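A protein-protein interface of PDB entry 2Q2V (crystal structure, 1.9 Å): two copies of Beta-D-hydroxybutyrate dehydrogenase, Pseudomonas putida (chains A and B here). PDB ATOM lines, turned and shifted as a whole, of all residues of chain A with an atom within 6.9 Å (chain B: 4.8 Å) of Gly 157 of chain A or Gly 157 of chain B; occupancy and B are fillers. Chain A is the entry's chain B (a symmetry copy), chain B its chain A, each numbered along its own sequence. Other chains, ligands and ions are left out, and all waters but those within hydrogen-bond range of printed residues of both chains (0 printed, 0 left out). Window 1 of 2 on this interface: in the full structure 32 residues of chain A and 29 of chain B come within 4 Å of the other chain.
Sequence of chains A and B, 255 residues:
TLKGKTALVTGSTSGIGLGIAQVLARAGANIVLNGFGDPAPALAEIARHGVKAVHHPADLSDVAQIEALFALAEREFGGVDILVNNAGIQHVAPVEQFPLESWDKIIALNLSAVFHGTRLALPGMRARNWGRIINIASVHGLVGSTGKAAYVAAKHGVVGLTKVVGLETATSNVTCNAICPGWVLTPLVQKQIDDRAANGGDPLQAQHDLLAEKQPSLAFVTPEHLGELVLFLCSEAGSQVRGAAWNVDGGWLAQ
NZ of Lys 163 of chain A sits at hydrogen-bond distance from NE2 of His 156 of chain B, at 2.9 Å.
The backbone carbonyl oxygen (O) of Val 152 of chain B sits at hydrogen-bond distance from a ring nitrogen (ND1) of His 156 of chain B, at 3.0 Å. The backbone carbonyl oxygen (O) of His 140 of chain A sits close to a ring nitrogen (NE2) of His 156 of chain A, at 3.4 Å. O of Gly 141 of chain A lies close to ND1 of His 156 of chain A (3.4 Å).
Among the printed residues, merely in contact across the chains: His 156 of chain A with His 156 of chain B, Ala 153 of chain A with Gly 157 of chain B, Gly 157 of chain A with Ala 153 of chain B, Gly 160 of chain A with Val 152 of chain B, Gly 160 of chain A with His 156 of chain B, His 156 of chain A with Gly 160 of chain B, Val 152 of chain A with Gly 160 of chain B, Ala 149 of chain A with Leu 161 of chain B and Gly 157 of chain A with Gly 157 of chain B.
Of the printed residues of chain B, Val 152 of chain A touches Gly 160. Of the printed residues of chain B, Ala 153 of chain A touches Gly 157 (3.2 Å). Gly 157 of chain A touches just these residues of chain B: Ala 153 and Gly 157. Printed residues of chain A within 4 Å of His 156 of chain B: His 156 (3.1 Å), Gly 160 (3.4 Å) and Lys 163 (2.9 Å). Gly 157 of chain B touches two residues of chain A.
Hydrophobic or aromatic side chains of chain B within 4 Å of the printed part of chain A: Val 152, Ala 153, His 156 and Leu 161. Among the printed residues, 10 pairs touch across the chains. Among the printed residues, no Asp or Glu carboxylate lies within 4 Å of a Lys or Arg side-chain nitrogen of the other chain.
Val 152 of chain A touches Gly 160 of chain B, and with the chains exchanged Gly 160 of chain A touches Val 152 of chain B. Ala 153 of chain A touches Gly 157 of chain B, and with the chains exchanged Gly 157 of chain A touches Ala 153 of chain B. His 156 of chain A touches Gly 160 of chain B, and with the chains exchanged Gly 160 of chain A touches His 156 of chain B. Gly 157 of chain B touches its own counterpart, Gly 157 of chain A. 11 positions are printed for both chains. Of the 10 pairs that touch across the chains among the printed residues, 8 have their exchanged pair printed and touching as well.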
ATOM      1  N   TRP A 103      13.244 -13.881   5.596  1.00  0.00           N
ATOM      2  CA  TRP A 103      12.061 -13.010   5.410  1.00  0.00           C
ATOM      3  C   TRP A 103      11.177 -13.173   6.670  1.00  0.00           C
ATOM      4  O   TRP A 103      10.891 -12.195   7.326  1.00  0.00           O
ATOM      5  CB  TRP A 103      11.275 -13.377   4.128  1.00  0.00           C
ATOM      6  CG  TRP A 103       9.938 -12.638   4.080  1.00  0.00           C
ATOM      7  CD1 TRP A 103       8.757 -13.077   4.602  1.00  0.00           C
ATOM      8  CD2 TRP A 103       9.672 -11.344   3.512  1.00  0.00           C
ATOM      9  NE1 TRP A 103       7.777 -12.144   4.409  1.00  0.00           N
ATOM     10  CE2 TRP A 103       8.295 -11.069   3.735  1.00  0.00           C
ATOM     11  CE3 TRP A 103      10.457 -10.392   2.844  1.00  0.00           C
ATOM     12  CZ2 TRP A 103       7.678  -9.874   3.319  1.00  0.00           C
ATOM     13  CZ3 TRP A 103       9.841  -9.197   2.419  1.00  0.00           C
ATOM     14  CH2 TRP A 103       8.459  -8.941   2.687  1.00  0.00           C
ATOM     15  N   ASN A 110      11.254  -7.615  13.457  1.00  0.00           N
ATOM     16  CA  ASN A 110      11.346  -6.199  13.144  1.00  0.00           C
ATOM     17  C   ASN A 110       9.964  -5.543  12.985  1.00  0.00           C
ATOM     18  O   ASN A 110       9.861  -4.313  12.998  1.00  0.00           O
ATOM     19  CB  ASN A 110      12.209  -5.906  11.899  1.00  0.00           C
ATOM     20  CG  ASN A 110      13.716  -6.233  12.088  1.00  0.00           C
ATOM     21  OD1 ASN A 110      14.583  -5.745  11.315  1.00  0.00           O
ATOM     22  ND2 ASN A 110      14.024  -7.063  13.033  1.00  0.00           N
ATOM     23  N   LEU A 111       8.922  -6.347  12.805  1.00  0.00           N
ATOM     24  CA  LEU A 111       7.560  -5.789  12.681  1.00  0.00           C
ATOM     25  C   LEU A 111       6.592  -6.388  13.692  1.00  0.00           C
ATOM     26  O   LEU A 111       6.025  -5.655  14.526  1.00  0.00           O
ATOM     27  CB  LEU A 111       7.015  -5.913  11.239  1.00  0.00           C
ATOM     28  CG  LEU A 111       5.533  -5.518  10.970  1.00  0.00           C
ATOM     29  CD1 LEU A 111       5.217  -4.130  11.450  1.00  0.00           C
ATOM     30  CD2 LEU A 111       5.212  -5.639   9.470  1.00  0.00           C
ATOM     31  N   HIS A 140      15.115   3.334   6.591  1.00  0.00           N
ATOM     32  CA  HIS A 140      14.523   2.261   5.752  1.00  0.00           C
ATOM     33  C   HIS A 140      13.047   1.994   6.020  1.00  0.00           C
ATOM     34  O   HIS A 140      12.438   1.088   5.416  1.00  0.00           O
ATOM     35  CB  HIS A 140      15.345   0.972   5.851  1.00  0.00           C
ATOM     36  CG  HIS A 140      16.703   1.084   5.236  1.00  0.00           C
ATOM     37  ND1 HIS A 140      16.899   1.429   3.916  1.00  0.00           N
ATOM     38  CD2 HIS A 140      17.934   0.892   5.763  1.00  0.00           C
ATOM     39  CE1 HIS A 140      18.196   1.434   3.655  1.00  0.00           C
ATOM     40  NE2 HIS A 140      18.845   1.111   4.757  1.00  0.00           N
ATOM     41  N   GLY A 141      12.456   2.781   6.921  1.00  0.00           N
ATOM     42  CA  GLY A 141      10.995   2.849   7.044  1.00  0.00           C
ATOM     43  C   GLY A 141      10.375   3.883   6.117  1.00  0.00           C
ATOM     44  O   GLY A 141       9.151   4.013   6.035  1.00  0.00           O
ATOM     45  N   ALA A 149      15.088  -6.296   1.176  1.00  0.00           N
ATOM     46  CA  ALA A 149      13.628  -6.540   1.027  1.00  0.00           C
ATOM     47  C   ALA A 149      12.871  -6.671   2.359  1.00  0.00           C
ATOM     48  O   ALA A 149      11.898  -5.933   2.607  1.00  0.00           O
ATOM     49  CB  ALA A 149      13.357  -7.773   0.158  1.00  0.00           C
ATOM     50  N   TYR A 151      13.835  -6.242   5.558  1.00  0.00           N
ATOM     51  CA  TYR A 151      14.089  -5.179   6.548  1.00  0.00           C
ATOM     52  C   TYR A 151      13.330  -3.894   6.192  1.00  0.00           C
ATOM     53  O   TYR A 151      12.617  -3.310   7.041  1.00  0.00           O
ATOM     54  CB  TYR A 151      15.586  -4.929   6.634  1.00  0.00           C
ATOM     55  CG  TYR A 151      16.044  -3.926   7.663  1.00  0.00           C
ATOM     56  CD1 TYR A 151      16.137  -2.592   7.358  1.00  0.00           C
ATOM     57  CD2 TYR A 151      16.487  -4.357   8.940  1.00  0.00           C
ATOM     58  CE1 TYR A 151      16.618  -1.685   8.292  1.00  0.00           C
ATOM     59  CE2 TYR A 151      16.903  -3.463   9.888  1.00  0.00           C
ATOM     60  CZ  TYR A 151      17.012  -2.134   9.551  1.00  0.00           C
ATOM     61  OH  TYR A 151      17.487  -1.244  10.479  1.00  0.00           O
ATOM     62  N   VAL A 152      13.457  -3.457   4.935  1.00  0.00           N
ATOM     63  CA  VAL A 152      12.690  -2.272   4.475  1.00  0.00           C
ATOM     64  C   VAL A 152      11.178  -2.491   4.591  1.00  0.00           C
ATOM     65  O   VAL A 152      10.462  -1.585   5.018  1.00  0.00           O
ATOM     66  CB  VAL A 152      13.054  -1.859   3.024  1.00  0.00           C
ATOM     67  CG1 VAL A 152      12.179  -0.702   2.543  1.00  0.00           C
ATOM     68  CG2 VAL A 152      14.545  -1.464   2.980  1.00  0.00           C
ATOM     69  N   ALA A 153      10.671  -3.663   4.197  1.00  0.00           N
ATOM     70  CA  ALA A 153       9.246  -3.929   4.395  1.00  0.00           C
ATOM     71  C   ALA A 153       8.845  -3.783   5.862  1.00  0.00           C
ATOM     72  O   ALA A 153       7.824  -3.141   6.192  1.00  0.00           O
ATOM     73  CB  ALA A 153       8.854  -5.323   3.893  1.00  0.00           C
ATOM     74  N   ALA A 154       9.588  -4.462   6.734  1.00  0.00           N
ATOM     75  CA  ALA A 154       9.275  -4.436   8.179  1.00  0.00           C
ATOM     76  C   ALA A 154       9.289  -3.009   8.771  1.00  0.00           C
ATOM     77  O   ALA A 154       8.387  -2.619   9.534  1.00  0.00           O
ATOM     78  CB  ALA A 154      10.286  -5.313   8.925  1.00  0.00           C
ATOM     79  N   LYS A 155      10.341  -2.264   8.431  1.00  0.00           N
ATOM     80  CA  LYS A 155      10.524  -0.872   8.892  1.00  0.00           C
ATOM     81  C   LYS A 155       9.457   0.097   8.361  1.00  0.00           C
ATOM     82  O   LYS A 155       8.954   0.919   9.128  1.00  0.00           O
ATOM     83  CB  LYS A 155      11.945  -0.402   8.612  1.00  0.00           C
ATOM     84  CG  LYS A 155      13.038  -1.212   9.381  1.00  0.00           C
ATOM     85  CD  LYS A 155      12.957  -0.929  10.891  1.00  0.00           C
ATOM     86  CE  LYS A 155      14.145  -1.647  11.625  1.00  0.00           C
ATOM     87  NZ  LYS A 155      14.106  -1.341  13.116  1.00  0.00           N
ATOM     88  N   HIS A 156       9.089  -0.012   7.082  1.00  0.00           N
ATOM     89  CA  HIS A 156       7.869   0.672   6.593  1.00  0.00           C
ATOM     90  C   HIS A 156       6.633   0.244   7.368  1.00  0.00           C
ATOM     91  O   HIS A 156       5.795   1.061   7.729  1.00  0.00           O
ATOM     92  CB  HIS A 156       7.663   0.398   5.095  1.00  0.00           C
ATOM     93  CG  HIS A 156       8.551   1.229   4.228  1.00  0.00           C
ATOM     94  ND1 HIS A 156       8.070   2.199   3.372  1.00  0.00           N
ATOM     95  CD2 HIS A 156       9.900   1.240   4.095  1.00  0.00           C
ATOM     96  CE1 HIS A 156       9.083   2.761   2.732  1.00  0.00           C
ATOM     97  NE2 HIS A 156      10.202   2.234   3.182  1.00  0.00           N
ATOM     98  N   GLY A 157       6.500  -1.062   7.615  1.00  0.00           N
ATOM     99  CA  GLY A 157       5.375  -1.527   8.464  1.00  0.00           C
ATOM    100  C   GLY A 157       5.321  -0.843   9.831  1.00  0.00           C
ATOM    101  O   GLY A 157       4.239  -0.448  10.321  1.00  0.00           O
ATOM    102  N   VAL A 158       6.483  -0.716  10.452  1.00  0.00           N
ATOM    103  CA  VAL A 158       6.598  -0.060  11.748  1.00  0.00           C
ATOM    104  C   VAL A 158       6.177   1.405  11.674  1.00  0.00           C
ATOM    105  O   VAL A 158       5.426   1.905  12.533  1.00  0.00           O
ATOM    106  CB  VAL A 158       8.027  -0.178  12.312  1.00  0.00           C
ATOM    107  CG1 VAL A 158       8.162   0.671  13.584  1.00  0.00           C
ATOM    108  CG2 VAL A 158       8.302  -1.645  12.663  1.00  0.00           C
ATOM    109  N   VAL A 159       6.596   2.084  10.618  1.00  0.00           N
ATOM    110  CA  VAL A 159       6.216   3.472  10.454  1.00  0.00           C
ATOM    111  C   VAL A 159       4.671   3.588  10.262  1.00  0.00           C
ATOM    112  O   VAL A 159       4.037   4.434  10.882  1.00  0.00           O
ATOM    113  CB  VAL A 159       7.006   4.112   9.307  1.00  0.00           C
ATOM    114  CG1 VAL A 159       6.393   5.469   8.914  1.00  0.00           C
ATOM    115  CG2 VAL A 159       8.479   4.265   9.741  1.00  0.00           C
ATOM    116  N   GLY A 160       4.070   2.694   9.472  1.00  0.00           N
ATOM    117  CA  GLY A 160       2.605   2.667   9.358  1.00  0.00           C
ATOM    118  C   GLY A 160       1.912   2.301  10.668  1.00  0.00           C
ATOM    119  O   GLY A 160       0.928   2.930  11.054  1.00  0.00           O
ATOM    120  N   LEU A 161       2.372   1.246  11.335  1.00  0.00           N
ATOM    121  CA  LEU A 161       1.780   0.857  12.641  1.00  0.00           C
ATOM    122  C   LEU A 161       1.758   2.067  13.607  1.00  0.00           C
ATOM    123  O   LEU A 161       0.774   2.306  14.335  1.00  0.00           O
ATOM    124  CB  LEU A 161       2.607  -0.256  13.296  1.00  0.00           C
ATOM    125  CG  LEU A 161       2.147  -0.795  14.688  1.00  0.00           C
ATOM    126  CD1 LEU A 161       0.725  -1.347  14.727  1.00  0.00           C
ATOM    127  CD2 LEU A 161       3.141  -1.833  15.155  1.00  0.00           C
ATOM    128  N   THR A 162       2.884   2.778  13.626  1.00  0.00           N
ATOM    129  CA  THR A 162       3.093   3.959  14.481  1.00  0.00           C
ATOM    130  C   THR A 162       2.005   4.998  14.260  1.00  0.00           C
ATOM    131  O   THR A 162       1.465   5.558  15.209  1.00  0.00           O
ATOM    132  CB  THR A 162       4.511   4.535  14.244  1.00  0.00           C
ATOM    133  OG1 THR A 162       5.504   3.537  14.630  1.00  0.00           O
ATOM    134  CG2 THR A 162       4.732   5.818  15.045  1.00  0.00           C
ATOM    135  N   LYS A 163       1.658   5.243  12.990  1.00  0.00           N
ATOM    136  CA  LYS A 163       0.561   6.174  12.688  1.00  0.00           C
ATOM    137  C   LYS A 163      -0.758   5.710  13.262  1.00  0.00           C
ATOM    138  O   LYS A 163      -1.480   6.514  13.839  1.00  0.00           O
ATOM    139  CB  LYS A 163       0.439   6.387  11.163  1.00  0.00           C
ATOM    140  CG  LYS A 163       1.729   6.921  10.514  1.00  0.00           C
ATOM    141  CD  LYS A 163       1.677   6.867   8.956  1.00  0.00           C
ATOM    142  CE  LYS A 163       3.064   7.293   8.348  1.00  0.00           C
ATOM    143  NZ  LYS A 163       3.124   7.000   6.874  1.00  0.00           N
ATOM    144  N   LEU B 111       1.072  -8.648   2.662  1.00  0.00           N
ATOM    145  CA  LEU B 111       2.503  -8.329   2.596  1.00  0.00           C
ATOM    146  C   LEU B 111       3.353  -9.489   2.108  1.00  0.00           C
ATOM    147  O   LEU B 111       4.000  -9.373   1.048  1.00  0.00           O
ATOM    148  CB  LEU B 111       3.026  -7.715   3.937  1.00  0.00           C
ATOM    149  CG  LEU B 111       4.540  -7.450   3.984  1.00  0.00           C
ATOM    150  CD1 LEU B 111       5.034  -6.565   2.771  1.00  0.00           C
ATOM    151  CD2 LEU B 111       4.913  -6.837   5.314  1.00  0.00           C
ATOM    152  N   VAL B 152      -2.655  -1.398   7.711  1.00  0.00           N
ATOM    153  CA  VAL B 152      -1.722  -0.267   7.481  1.00  0.00           C
ATOM    154  C   VAL B 152      -0.284  -0.734   7.528  1.00  0.00           C
ATOM    155  O   VAL B 152       0.493  -0.375   6.654  1.00  0.00           O
ATOM    156  CB  VAL B 152      -1.997   0.889   8.473  1.00  0.00           C
ATOM    157  CG1 VAL B 152      -0.942   2.013   8.363  1.00  0.00           C
ATOM    158  CG2 VAL B 152      -3.447   1.426   8.182  1.00  0.00           C
ATOM    159  N   ALA B 153       0.064  -1.562   8.520  1.00  0.00           N
ATOM    160  CA  ALA B 153       1.431  -2.113   8.564  1.00  0.00           C
ATOM    161  C   ALA B 153       1.759  -2.876   7.283  1.00  0.00           C
ATOM    162  O   ALA B 153       2.811  -2.663   6.711  1.00  0.00           O
ATOM    163  CB  ALA B 153       1.627  -3.007   9.743  1.00  0.00           C
ATOM    164  N   ALA B 154       0.875  -3.808   6.896  1.00  0.00           N
ATOM    165  CA  ALA B 154       1.082  -4.652   5.733  1.00  0.00           C
ATOM    166  C   ALA B 154       1.223  -3.799   4.467  1.00  0.00           C
ATOM    167  O   ALA B 154       2.186  -3.985   3.710  1.00  0.00           O
ATOM    168  CB  ALA B 154      -0.018  -5.670   5.597  1.00  0.00           C
ATOM    169  N   LYS B 155       0.300  -2.865   4.262  1.00  0.00           N
ATOM    170  CA  LYS B 155       0.341  -1.999   3.053  1.00  0.00           C
ATOM    171  C   LYS B 155       1.580  -1.053   3.022  1.00  0.00           C
ATOM    172  O   LYS B 155       2.211  -0.849   1.982  1.00  0.00           O
ATOM    173  CB  LYS B 155      -0.974  -1.240   2.903  1.00  0.00           C
ATOM    174  CG  LYS B 155      -2.189  -2.169   2.605  1.00  0.00           C
ATOM    175  CD  LYS B 155      -2.059  -2.895   1.235  1.00  0.00           C
ATOM    176  CE  LYS B 155      -3.432  -3.541   0.869  1.00  0.00           C
ATOM    177  NZ  LYS B 155      -3.326  -4.264  -0.411  1.00  0.00           N
ATOM    178  N   HIS B 156       1.952  -0.501   4.171  1.00  0.00           N
ATOM    179  CA  HIS B 156       3.231   0.246   4.254  1.00  0.00           C
ATOM    180  C   HIS B 156       4.416  -0.679   3.887  1.00  0.00           C
ATOM    181  O   HIS B 156       5.312  -0.304   3.129  1.00  0.00           O
ATOM    182  CB  HIS B 156       3.446   0.823   5.687  1.00  0.00           C
ATOM    183  CG  HIS B 156       2.837   2.187   5.900  1.00  0.00           C
ATOM    184  ND1 HIS B 156       1.470   2.400   5.949  1.00  0.00           N
ATOM    185  CD2 HIS B 156       3.410   3.394   6.105  1.00  0.00           C
ATOM    186  CE1 HIS B 156       1.235   3.686   6.159  1.00  0.00           C
ATOM    187  NE2 HIS B 156       2.394   4.302   6.288  1.00  0.00           N
ATOM    188  N   GLY B 157       4.396  -1.905   4.401  1.00  0.00           N
ATOM    189  CA  GLY B 157       5.443  -2.886   4.053  1.00  0.00           C
ATOM    190  C   GLY B 157       5.550  -3.115   2.555  1.00  0.00           C
ATOM    191  O   GLY B 157       6.657  -3.246   2.007  1.00  0.00           O
ATOM    192  N   VAL B 158       4.406  -3.184   1.890  1.00  0.00           N
ATOM    193  CA  VAL B 158       4.353  -3.348   0.435  1.00  0.00           C
ATOM    194  C   VAL B 158       4.975  -2.180  -0.302  1.00  0.00           C
ATOM    195  O   VAL B 158       5.735  -2.350  -1.277  1.00  0.00           O
ATOM    196  CB  VAL B 158       2.864  -3.532  -0.057  1.00  0.00           C
ATOM    197  CG1 VAL B 158       2.779  -3.502  -1.601  1.00  0.00           C
ATOM    198  CG2 VAL B 158       2.307  -4.821   0.454  1.00  0.00           C
ATOM    199  N   VAL B 159       4.635  -0.980   0.137  1.00  0.00           N
ATOM    200  CA  VAL B 159       5.271   0.230  -0.412  1.00  0.00           C
ATOM    201  C   VAL B 159       6.808   0.196  -0.247  1.00  0.00           C
ATOM    202  O   VAL B 159       7.555   0.495  -1.200  1.00  0.00           O
ATOM    203  CB  VAL B 159       4.595   1.496   0.170  1.00  0.00           C
ATOM    204  CG1 VAL B 159       5.500   2.814   0.022  1.00  0.00           C
ATOM    205  CG2 VAL B 159       3.211   1.669  -0.473  1.00  0.00           C
ATOM    206  N   GLY B 160       7.283  -0.193   0.929  1.00  0.00           N
ATOM    207  CA  GLY B 160       8.727  -0.381   1.142  1.00  0.00           C
ATOM    208  C   GLY B 160       9.344  -1.451   0.257  1.00  0.00           C
ATOM    209  O   GLY B 160      10.347  -1.216  -0.393  1.00  0.00           O
ATOM    210  N   LEU B 161       8.751  -2.642   0.251  1.00  0.00           N
ATOM    211  CA  LEU B 161       9.213  -3.743  -0.616  1.00  0.00           C
ATOM    212  C   LEU B 161       9.291  -3.314  -2.098  1.00  0.00           C
ATOM    213  O   LEU B 161      10.283  -3.624  -2.798  1.00  0.00           O
ATOM    214  CB  LEU B 161       8.259  -4.949  -0.500  1.00  0.00           C
ATOM    215  CG  LEU B 161       8.573  -6.162  -1.394  1.00  0.00           C
ATOM    216  CD1 LEU B 161      10.025  -6.633  -1.128  1.00  0.00           C
ATOM    217  CD2 LEU B 161       7.570  -7.238  -1.099  1.00  0.00           C
